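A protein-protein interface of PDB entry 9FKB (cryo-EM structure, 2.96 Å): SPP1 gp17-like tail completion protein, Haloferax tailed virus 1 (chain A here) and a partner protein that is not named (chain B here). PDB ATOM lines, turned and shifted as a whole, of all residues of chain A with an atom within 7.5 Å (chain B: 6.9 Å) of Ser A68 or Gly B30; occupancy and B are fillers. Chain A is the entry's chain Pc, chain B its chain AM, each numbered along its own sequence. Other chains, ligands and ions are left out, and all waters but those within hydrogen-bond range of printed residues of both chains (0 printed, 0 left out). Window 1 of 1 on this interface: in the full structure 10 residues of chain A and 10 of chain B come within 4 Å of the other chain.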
ATOM      1  N   ASP A  65       0.311  22.910 -11.424  1.00  0.00           N
ATOM      2  CA  ASP A  65      -0.073  21.634 -12.014  1.00  0.00           C
ATOM      3  C   ASP A  65      -1.584  21.535 -12.213  1.00  0.00           C
ATOM      4  O   ASP A  65      -2.379  22.009 -11.393  1.00  0.00           O
ATOM      5  CB  ASP A  65       0.442  20.458 -11.191  1.00  0.00           C
ATOM      6  CG  ASP A  65       1.924  20.142 -11.356  1.00  0.00           C
ATOM      7  OD1 ASP A  65       2.619  20.870 -12.101  1.00  0.00           O
ATOM      8  OD2 ASP A  65       2.384  19.155 -10.731  1.00  0.00           O
ATOM      9  N   ARG A  66      -1.977  20.855 -13.303  1.00  0.00           N
ATOM     10  CA  ARG A  66      -3.368  20.494 -13.526  1.00  0.00           C
ATOM     11  C   ARG A  66      -3.790  19.527 -12.422  1.00  0.00           C
ATOM     12  O   ARG A  66      -3.071  18.557 -12.133  1.00  0.00           O
ATOM     13  CB  ARG A  66      -3.516  19.845 -14.909  1.00  0.00           C
ATOM     14  CG  ARG A  66      -3.318  20.808 -16.071  1.00  0.00           C
ATOM     15  CD  ARG A  66      -4.439  21.849 -16.149  1.00  0.00           C
ATOM     16  NE  ARG A  66      -5.810  21.373 -16.248  1.00  0.00           N
ATOM     17  CZ  ARG A  66      -6.535  21.306 -17.369  1.00  0.00           C
ATOM     18  NH1 ARG A  66      -7.774  20.866 -17.304  1.00  0.00           N
ATOM     19  NH2 ARG A  66      -6.071  21.708 -18.549  1.00  0.00           N
ATOM     20  N   PHE A  67      -4.976  19.749 -11.836  1.00  0.00           N
ATOM     21  CA  PHE A  67      -5.434  18.834 -10.794  1.00  0.00           C
ATOM     22  C   PHE A  67      -6.264  17.664 -11.343  1.00  0.00           C
ATOM     23  O   PHE A  67      -6.224  16.548 -10.822  1.00  0.00           O
ATOM     24  CB  PHE A  67      -6.267  19.599  -9.782  1.00  0.00           C
ATOM     25  CG  PHE A  67      -6.620  18.807  -8.551  1.00  0.00           C
ATOM     26  CD1 PHE A  67      -5.619  18.335  -7.696  1.00  0.00           C
ATOM     27  CD2 PHE A  67      -7.957  18.571  -8.244  1.00  0.00           C
ATOM     28  CE1 PHE A  67      -5.943  17.606  -6.561  1.00  0.00           C
ATOM     29  CE2 PHE A  67      -8.284  17.861  -7.090  1.00  0.00           C
ATOM     30  CZ  PHE A  67      -7.276  17.385  -6.256  1.00  0.00           C
ATOM     31  N   SER A  68      -7.051  17.942 -12.393  1.00  0.00           N
ATOM     32  CA  SER A  68      -8.057  17.019 -12.899  1.00  0.00           C
ATOM     33  C   SER A  68      -8.562  17.472 -14.267  1.00  0.00           C
ATOM     34  O   SER A  68      -8.292  18.593 -14.690  1.00  0.00           O
ATOM     35  CB  SER A  68      -9.227  16.962 -11.936  1.00  0.00           C
ATOM     36  OG  SER A  68      -9.972  18.175 -11.936  1.00  0.00           O
ATOM     37  N   MET A  69      -9.391  16.651 -14.927  1.00  0.00           N
ATOM     38  CA  MET A  69      -9.971  17.045 -16.203  1.00  0.00           C
ATOM     39  C   MET A  69     -10.970  18.190 -16.054  1.00  0.00           C
ATOM     40  O   MET A  69     -11.368  18.784 -17.057  1.00  0.00           O
ATOM     41  CB  MET A  69     -10.642  15.847 -16.877  1.00  0.00           C
ATOM     42  CG  MET A  69      -9.612  14.893 -17.467  1.00  0.00           C
ATOM     43  SD  MET A  69     -10.205  13.222 -17.830  1.00  0.00           S
ATOM     44  CE  MET A  69     -11.580  13.637 -18.910  1.00  0.00           C
ATOM     45  N   ASP A  70     -11.400  18.519 -14.822  1.00  0.00           N
ATOM     46  CA  ASP A  70     -12.330  19.631 -14.629  1.00  0.00           C
ATOM     47  C   ASP A  70     -11.717  20.959 -15.081  1.00  0.00           C
ATOM     48  O   ASP A  70     -12.437  21.842 -15.571  1.00  0.00           O
ATOM     49  CB  ASP A  70     -12.718  19.842 -13.169  1.00  0.00           C
ATOM     50  CG  ASP A  70     -13.542  18.734 -12.516  1.00  0.00           C
ATOM     51  OD1 ASP A  70     -13.947  17.758 -13.194  1.00  0.00           O
ATOM     52  OD2 ASP A  70     -13.802  18.868 -11.302  1.00  0.00           O
ATOM     53  N   GLY A  71     -10.401  21.115 -14.890  1.00  0.00           N
ATOM     54  CA  GLY A  71      -9.716  22.378 -15.127  1.00  0.00           C
ATOM     55  C   GLY A  71     -10.171  23.501 -14.191  1.00  0.00           C
ATOM     56  O   GLY A  71      -9.931  24.678 -14.463  1.00  0.00           O
ATOM     57  N   ASP A  72     -10.806  23.129 -13.074  1.00  0.00           N
ATOM     58  CA  ASP A  72     -11.454  24.037 -12.132  1.00  0.00           C
ATOM     59  C   ASP A  72     -10.493  24.553 -11.048  1.00  0.00           C
ATOM     60  O   ASP A  72     -10.748  25.569 -10.405  1.00  0.00           O
ATOM     61  CB  ASP A  72     -12.620  23.265 -11.529  1.00  0.00           C
ATOM     62  CG  ASP A  72     -13.334  24.005 -10.415  1.00  0.00           C
ATOM     63  OD1 ASP A  72     -13.852  25.115 -10.686  1.00  0.00           O
ATOM     64  OD2 ASP A  72     -13.447  23.433  -9.299  1.00  0.00           O
ATOM     65  N   VAL A  73      -9.371  23.856 -10.848  1.00  0.00           N
ATOM     66  CA  VAL A  73      -8.398  24.227  -9.824  1.00  0.00           C
ATOM     67  C   VAL A  73      -6.968  23.828 -10.219  1.00  0.00           C
ATOM     68  O   VAL A  73      -6.774  22.864 -10.953  1.00  0.00           O
ATOM     69  CB  VAL A  73      -8.845  23.630  -8.485  1.00  0.00           C
ATOM     70  CG1 VAL A  73      -8.417  22.181  -8.305  1.00  0.00           C
ATOM     71  CG2 VAL A  73      -8.423  24.496  -7.315  1.00  0.00           C
ATOM     72  N   PHE A  74      -5.970  24.589  -9.749  1.00  0.00           N
ATOM     73  CA  PHE A  74      -4.559  24.279  -9.919  1.00  0.00           C
ATOM     74  C   PHE A  74      -3.953  23.780  -8.607  1.00  0.00           C
ATOM     75  O   PHE A  74      -4.204  24.350  -7.551  1.00  0.00           O
ATOM     76  CB  PHE A  74      -3.761  25.538 -10.262  1.00  0.00           C
ATOM     77  CG  PHE A  74      -4.017  26.147 -11.618  1.00  0.00           C
ATOM     78  CD1 PHE A  74      -3.869  25.391 -12.774  1.00  0.00           C
ATOM     79  CD2 PHE A  74      -4.325  27.496 -11.747  1.00  0.00           C
ATOM     80  CE1 PHE A  74      -4.064  25.961 -14.028  1.00  0.00           C
ATOM     81  CE2 PHE A  74      -4.511  28.066 -13.001  1.00  0.00           C
ATOM     82  CZ  PHE A  74      -4.389  27.299 -14.143  1.00  0.00           C
ATOM     83  N   ASP A  75      -3.103  22.758  -8.698  1.00  0.00           N
ATOM     84  CA  ASP A  75      -2.269  22.311  -7.598  1.00  0.00           C
ATOM     85  C   ASP A  75      -1.024  23.191  -7.565  1.00  0.00           C
ATOM     86  O   ASP A  75      -0.028  22.883  -8.221  1.00  0.00           O
ATOM     87  CB  ASP A  75      -1.960  20.825  -7.787  1.00  0.00           C
ATOM     88  CG  ASP A  75      -1.089  20.118  -6.751  1.00  0.00           C
ATOM     89  OD1 ASP A  75      -0.539  20.745  -5.848  1.00  0.00           O
ATOM     90  OD2 ASP A  75      -0.985  18.880  -6.842  1.00  0.00           O
ATOM     91  N   ASN B  11      -9.452  16.387 -21.689  1.00  0.00           N
ATOM     92  CA  ASN B  11     -10.036  17.251 -20.686  1.00  0.00           C
ATOM     93  C   ASN B  11     -11.317  17.922 -21.165  1.00  0.00           C
ATOM     94  O   ASN B  11     -12.085  18.406 -20.336  1.00  0.00           O
ATOM     95  CB  ASN B  11      -9.039  18.316 -20.273  1.00  0.00           C
ATOM     96  CG  ASN B  11      -7.675  17.788 -19.866  1.00  0.00           C
ATOM     97  OD1 ASN B  11      -7.531  16.630 -19.489  1.00  0.00           O
ATOM     98  ND2 ASN B  11      -6.668  18.649 -19.893  1.00  0.00           N
ATOM     99  N   PHE B  28     -20.785  14.565  -9.067  1.00  0.00           N
ATOM    100  CA  PHE B  28     -19.514  13.876  -9.216  1.00  0.00           C
ATOM    101  C   PHE B  28     -18.604  14.728 -10.092  1.00  0.00           C
ATOM    102  O   PHE B  28     -19.081  15.396 -11.008  1.00  0.00           O
ATOM    103  CB  PHE B  28     -19.769  12.524  -9.873  1.00  0.00           C
ATOM    104  CG  PHE B  28     -18.596  11.585  -9.859  1.00  0.00           C
ATOM    105  CD1 PHE B  28     -18.285  10.823  -8.732  1.00  0.00           C
ATOM    106  CD2 PHE B  28     -17.808  11.457 -10.994  1.00  0.00           C
ATOM    107  CE1 PHE B  28     -17.190   9.964  -8.737  1.00  0.00           C
ATOM    108  CE2 PHE B  28     -16.719  10.589 -11.002  1.00  0.00           C
ATOM    109  CZ  PHE B  28     -16.426   9.837  -9.879  1.00  0.00           C
ATOM    110  N   ALA B  29     -17.297  14.723  -9.782  1.00  0.00           N
ATOM    111  CA  ALA B  29     -16.366  15.681 -10.362  1.00  0.00           C
ATOM    112  C   ALA B  29     -14.917  15.196 -10.255  1.00  0.00           C
ATOM    113  O   ALA B  29     -14.603  14.292  -9.496  1.00  0.00           O
ATOM    114  CB  ALA B  29     -16.533  17.016  -9.648  1.00  0.00           C
ATOM    115  N   GLY B  30     -14.009  15.878 -10.956  1.00  0.00           N
ATOM    116  CA  GLY B  30     -12.583  15.780 -10.697  1.00  0.00           C
ATOM    117  C   GLY B  30     -11.942  14.536 -11.278  1.00  0.00           C
ATOM    118  O   GLY B  30     -10.988  14.033 -10.688  1.00  0.00           O
ATOM    119  N   VAL B  31     -12.465  14.040 -12.407  1.00  0.00           N
ATOM    120  CA  VAL B  31     -11.916  12.842 -13.034  1.00  0.00           C
ATOM    121  C   VAL B  31     -10.523  13.108 -13.604  1.00  0.00           C
ATOM    122  O   VAL B  31     -10.206  14.207 -14.044  1.00  0.00           O
ATOM    123  CB  VAL B  31     -12.866  12.227 -14.080  1.00  0.00           C
ATOM    124  CG1 VAL B  31     -14.221  11.929 -13.459  1.00  0.00           C
ATOM    125  CG2 VAL B  31     -13.055  13.070 -15.326  1.00  0.00           C
ATOM    126  N   ARG B  32      -9.673  12.073 -13.563  1.00  0.00           N
ATOM    127  CA  ARG B  32      -8.337  12.080 -14.131  1.00  0.00           C
ATOM    128  C   ARG B  32      -8.265  11.123 -15.318  1.00  0.00           C
ATOM    129  O   ARG B  32      -7.650  11.452 -16.330  1.00  0.00           O
ATOM    130  CB  ARG B  32      -7.308  11.700 -13.073  1.00  0.00           C
ATOM    131  CG  ARG B  32      -7.115  12.792 -12.043  1.00  0.00           C
ATOM    132  CD  ARG B  32      -6.043  12.499 -11.013  1.00  0.00           C
ATOM    133  NE  ARG B  32      -5.755  13.695 -10.242  1.00  0.00           N
ATOM    134  CZ  ARG B  32      -5.023  13.805  -9.133  1.00  0.00           C
ATOM    135  NH1 ARG B  32      -4.883  14.997  -8.580  1.00  0.00           N
ATOM    136  NH2 ARG B  32      -4.421  12.775  -8.573  1.00  0.00           N
ATOM    137  N   ASP B  33      -8.920   9.960 -15.200  1.00  0.00           N
ATOM    138  CA  ASP B  33      -9.002   8.978 -16.274  1.00  0.00           C
ATOM    139  C   ASP B  33     -10.454   8.531 -16.415  1.00  0.00           C
ATOM    140  O   ASP B  33     -11.150   8.394 -15.411  1.00  0.00           O
ATOM    141  CB  ASP B  33      -8.194   7.710 -15.980  1.00  0.00           C
ATOM    142  CG  ASP B  33      -6.796   7.900 -15.393  1.00  0.00           C
ATOM    143  OD1 ASP B  33      -6.148   8.924 -15.709  1.00  0.00           O
ATOM    144  OD2 ASP B  33      -6.340   6.987 -14.656  1.00  0.00           O
ATOM    145  N   THR B  68     -10.659   7.050 -12.788  1.00  0.00           N
ATOM    146  CA  THR B  68      -9.803   7.574 -11.735  1.00  0.00           C
ATOM    147  C   THR B  68     -10.226   9.013 -11.458  1.00  0.00           C
ATOM    148  O   THR B  68     -10.438   9.756 -12.407  1.00  0.00           O
ATOM    149  CB  THR B  68      -8.340   7.621 -12.178  1.00  0.00           C
ATOM    150  OG1 THR B  68      -7.965   6.328 -12.657  1.00  0.00           O
ATOM    151  CG2 THR B  68      -7.404   7.990 -11.041  1.00  0.00           C
ATOM    152  N   TYR B  69     -10.360   9.413 -10.186  1.00  0.00           N
ATOM    153  CA  TYR B  69     -10.819  10.754  -9.869  1.00  0.00           C
ATOM    154  C   TYR B  69     -10.195  11.280  -8.570  1.00  0.00           C
ATOM    155  O   TYR B  69      -9.658  10.516  -7.762  1.00  0.00           O
ATOM    156  CB  TYR B  69     -12.345  10.779  -9.897  1.00  0.00           C
ATOM    157  CG  TYR B  69     -13.054  10.128  -8.733  1.00  0.00           C
ATOM    158  CD1 TYR B  69     -13.107   8.747  -8.583  1.00  0.00           C
ATOM    159  CD2 TYR B  69     -13.710  10.898  -7.782  1.00  0.00           C
ATOM    160  CE1 TYR B  69     -13.788   8.159  -7.524  1.00  0.00           C
ATOM    161  CE2 TYR B  69     -14.380  10.327  -6.713  1.00  0.00           C
ATOM    162  CZ  TYR B  69     -14.424   8.950  -6.576  1.00  0.00           C
ATOM    163  OH  TYR B  69     -15.095   8.393  -5.515  1.00  0.00           O
ATOM    164  N   ALA B  70     -10.279  12.607  -8.348  1.00  0.00           N
ATOM    165  CA  ALA B  70      -9.542  13.263  -7.272  1.00  0.00           C
ATOM    166  C   ALA B  70     -10.392  14.202  -6.402  1.00  0.00           C
ATOM    167  O   ALA B  70      -9.881  14.759  -5.430  1.00  0.00           O
ATOM    168  CB  ALA B  70      -8.338  13.961  -7.866  1.00  0.00           C
ATOM    169  N   LYS B  71     -11.683  14.391  -6.724  1.00  0.00           N
ATOM    170  CA  LYS B  71     -12.611  15.104  -5.849  1.00  0.00           C
ATOM    171  C   LYS B  71     -13.588  14.115  -5.208  1.00  0.00           C
ATOM    172  O   LYS B  71     -14.344  13.463  -5.915  1.00  0.00           O
ATOM    173  CB  LYS B  71     -13.380  16.175  -6.611  1.00  0.00           C
ATOM    174  CG  LYS B  71     -12.513  17.349  -7.027  1.00  0.00           C
ATOM    175  CD  LYS B  71     -13.166  18.396  -7.879  1.00  0.00           C
ATOM    176  CE  LYS B  71     -12.067  19.286  -8.488  1.00  0.00           C
ATOM    177  NZ  LYS B  71     -12.533  20.402  -9.362  1.00  0.00           N
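Phe A67 touches Ala B70 (CZ to O, 3.8 Å). CB of Ser A68 touches O of Gly B30 (3.6 Å). Val B31 touches Ser A68 (O to CB, 3.6 Å). Ala B29 touches Asp A70.
The side-chain hydroxyl (OG) of Ser A68 lies close to the backbone NH (N) of Asp A70, at 3.2 Å. The backbone carbonyl oxygen (O) of Gly B30 sits at hydrogen-bond distance from the backbone NH (N) of Ala B70, 2.8 Å away. The backbone NH (N) of Arg B32 lies within hydrogen-bond range of the backbone carbonyl oxygen (O) of Thr B68, at 2.7 Å.
Printed residues of chain B that touch a printed residue of chain A: Asn B11, Ala B29, Gly B30, Val B31, Arg B32, Ala B70 and Lys B71. Hydrophobic or aromatic side chains of chain B that line the printed part of chain A: Ala B29, Val B31 and Ala B70. Among the printed residues, 12 pairs touch across the chains. Among the printed residues, Asp or Glu carboxylates within 4 Å of a Lys or Arg side-chain nitrogen of the other chain: Asp A70 with Lys B71 (2.8 Å) and Asp A72 with Lys B71 (3.2 Å).
Of the printed residues of chain B, Phe A67 touches Arg B32 and Ala B70. Of chain B, only Gly B30 (3.6 Å) and Val B31 (3.6 Å) come within 4 Å of Ser A68. Of the printed residues of chain A, Ala B29 touches Asp A70. Gly B30 touches just these residues of chain A: Ser A68 and Asp A70.
The side-chain amide nitrogen (ND2) of Asn B11 sits close to the guanidinium group (NH2) of Arg A66 (3.4 Å). The backbone carbonyl oxygen of Phe A67 lies within hydrogen-bond range of the guanidinium group of Arg B32 (2.9 Å). The backbone carbonyl oxygen (O) of Val B31 lies within hydrogen-bond range of the backbone NH (N) of Met A69, at 2.7 Å. The side-chain carboxylate (OD1) of Asp A70 is in hydrogen-bond range of the backbone NH (N) of Gly B30 (2.9 Å). The side-chain amino group (NZ) of Lys B71 is in salt-bridge range of the side-chain carboxylate (OD2) of Asp A70 (2.8 Å). The side-chain amino group (NZ) of Lys B71 lies within salt-bridge range of the side-chain carboxylate (OD2) of Asp A72 (3.2 Å). O of Asn B11 lies close to O of Met A69, at 3.4 Å. The side-chain sulfur (SD) of Met A69 sits close to the backbone carbonyl oxygen (O) of Arg B32, at 3.5 Å.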
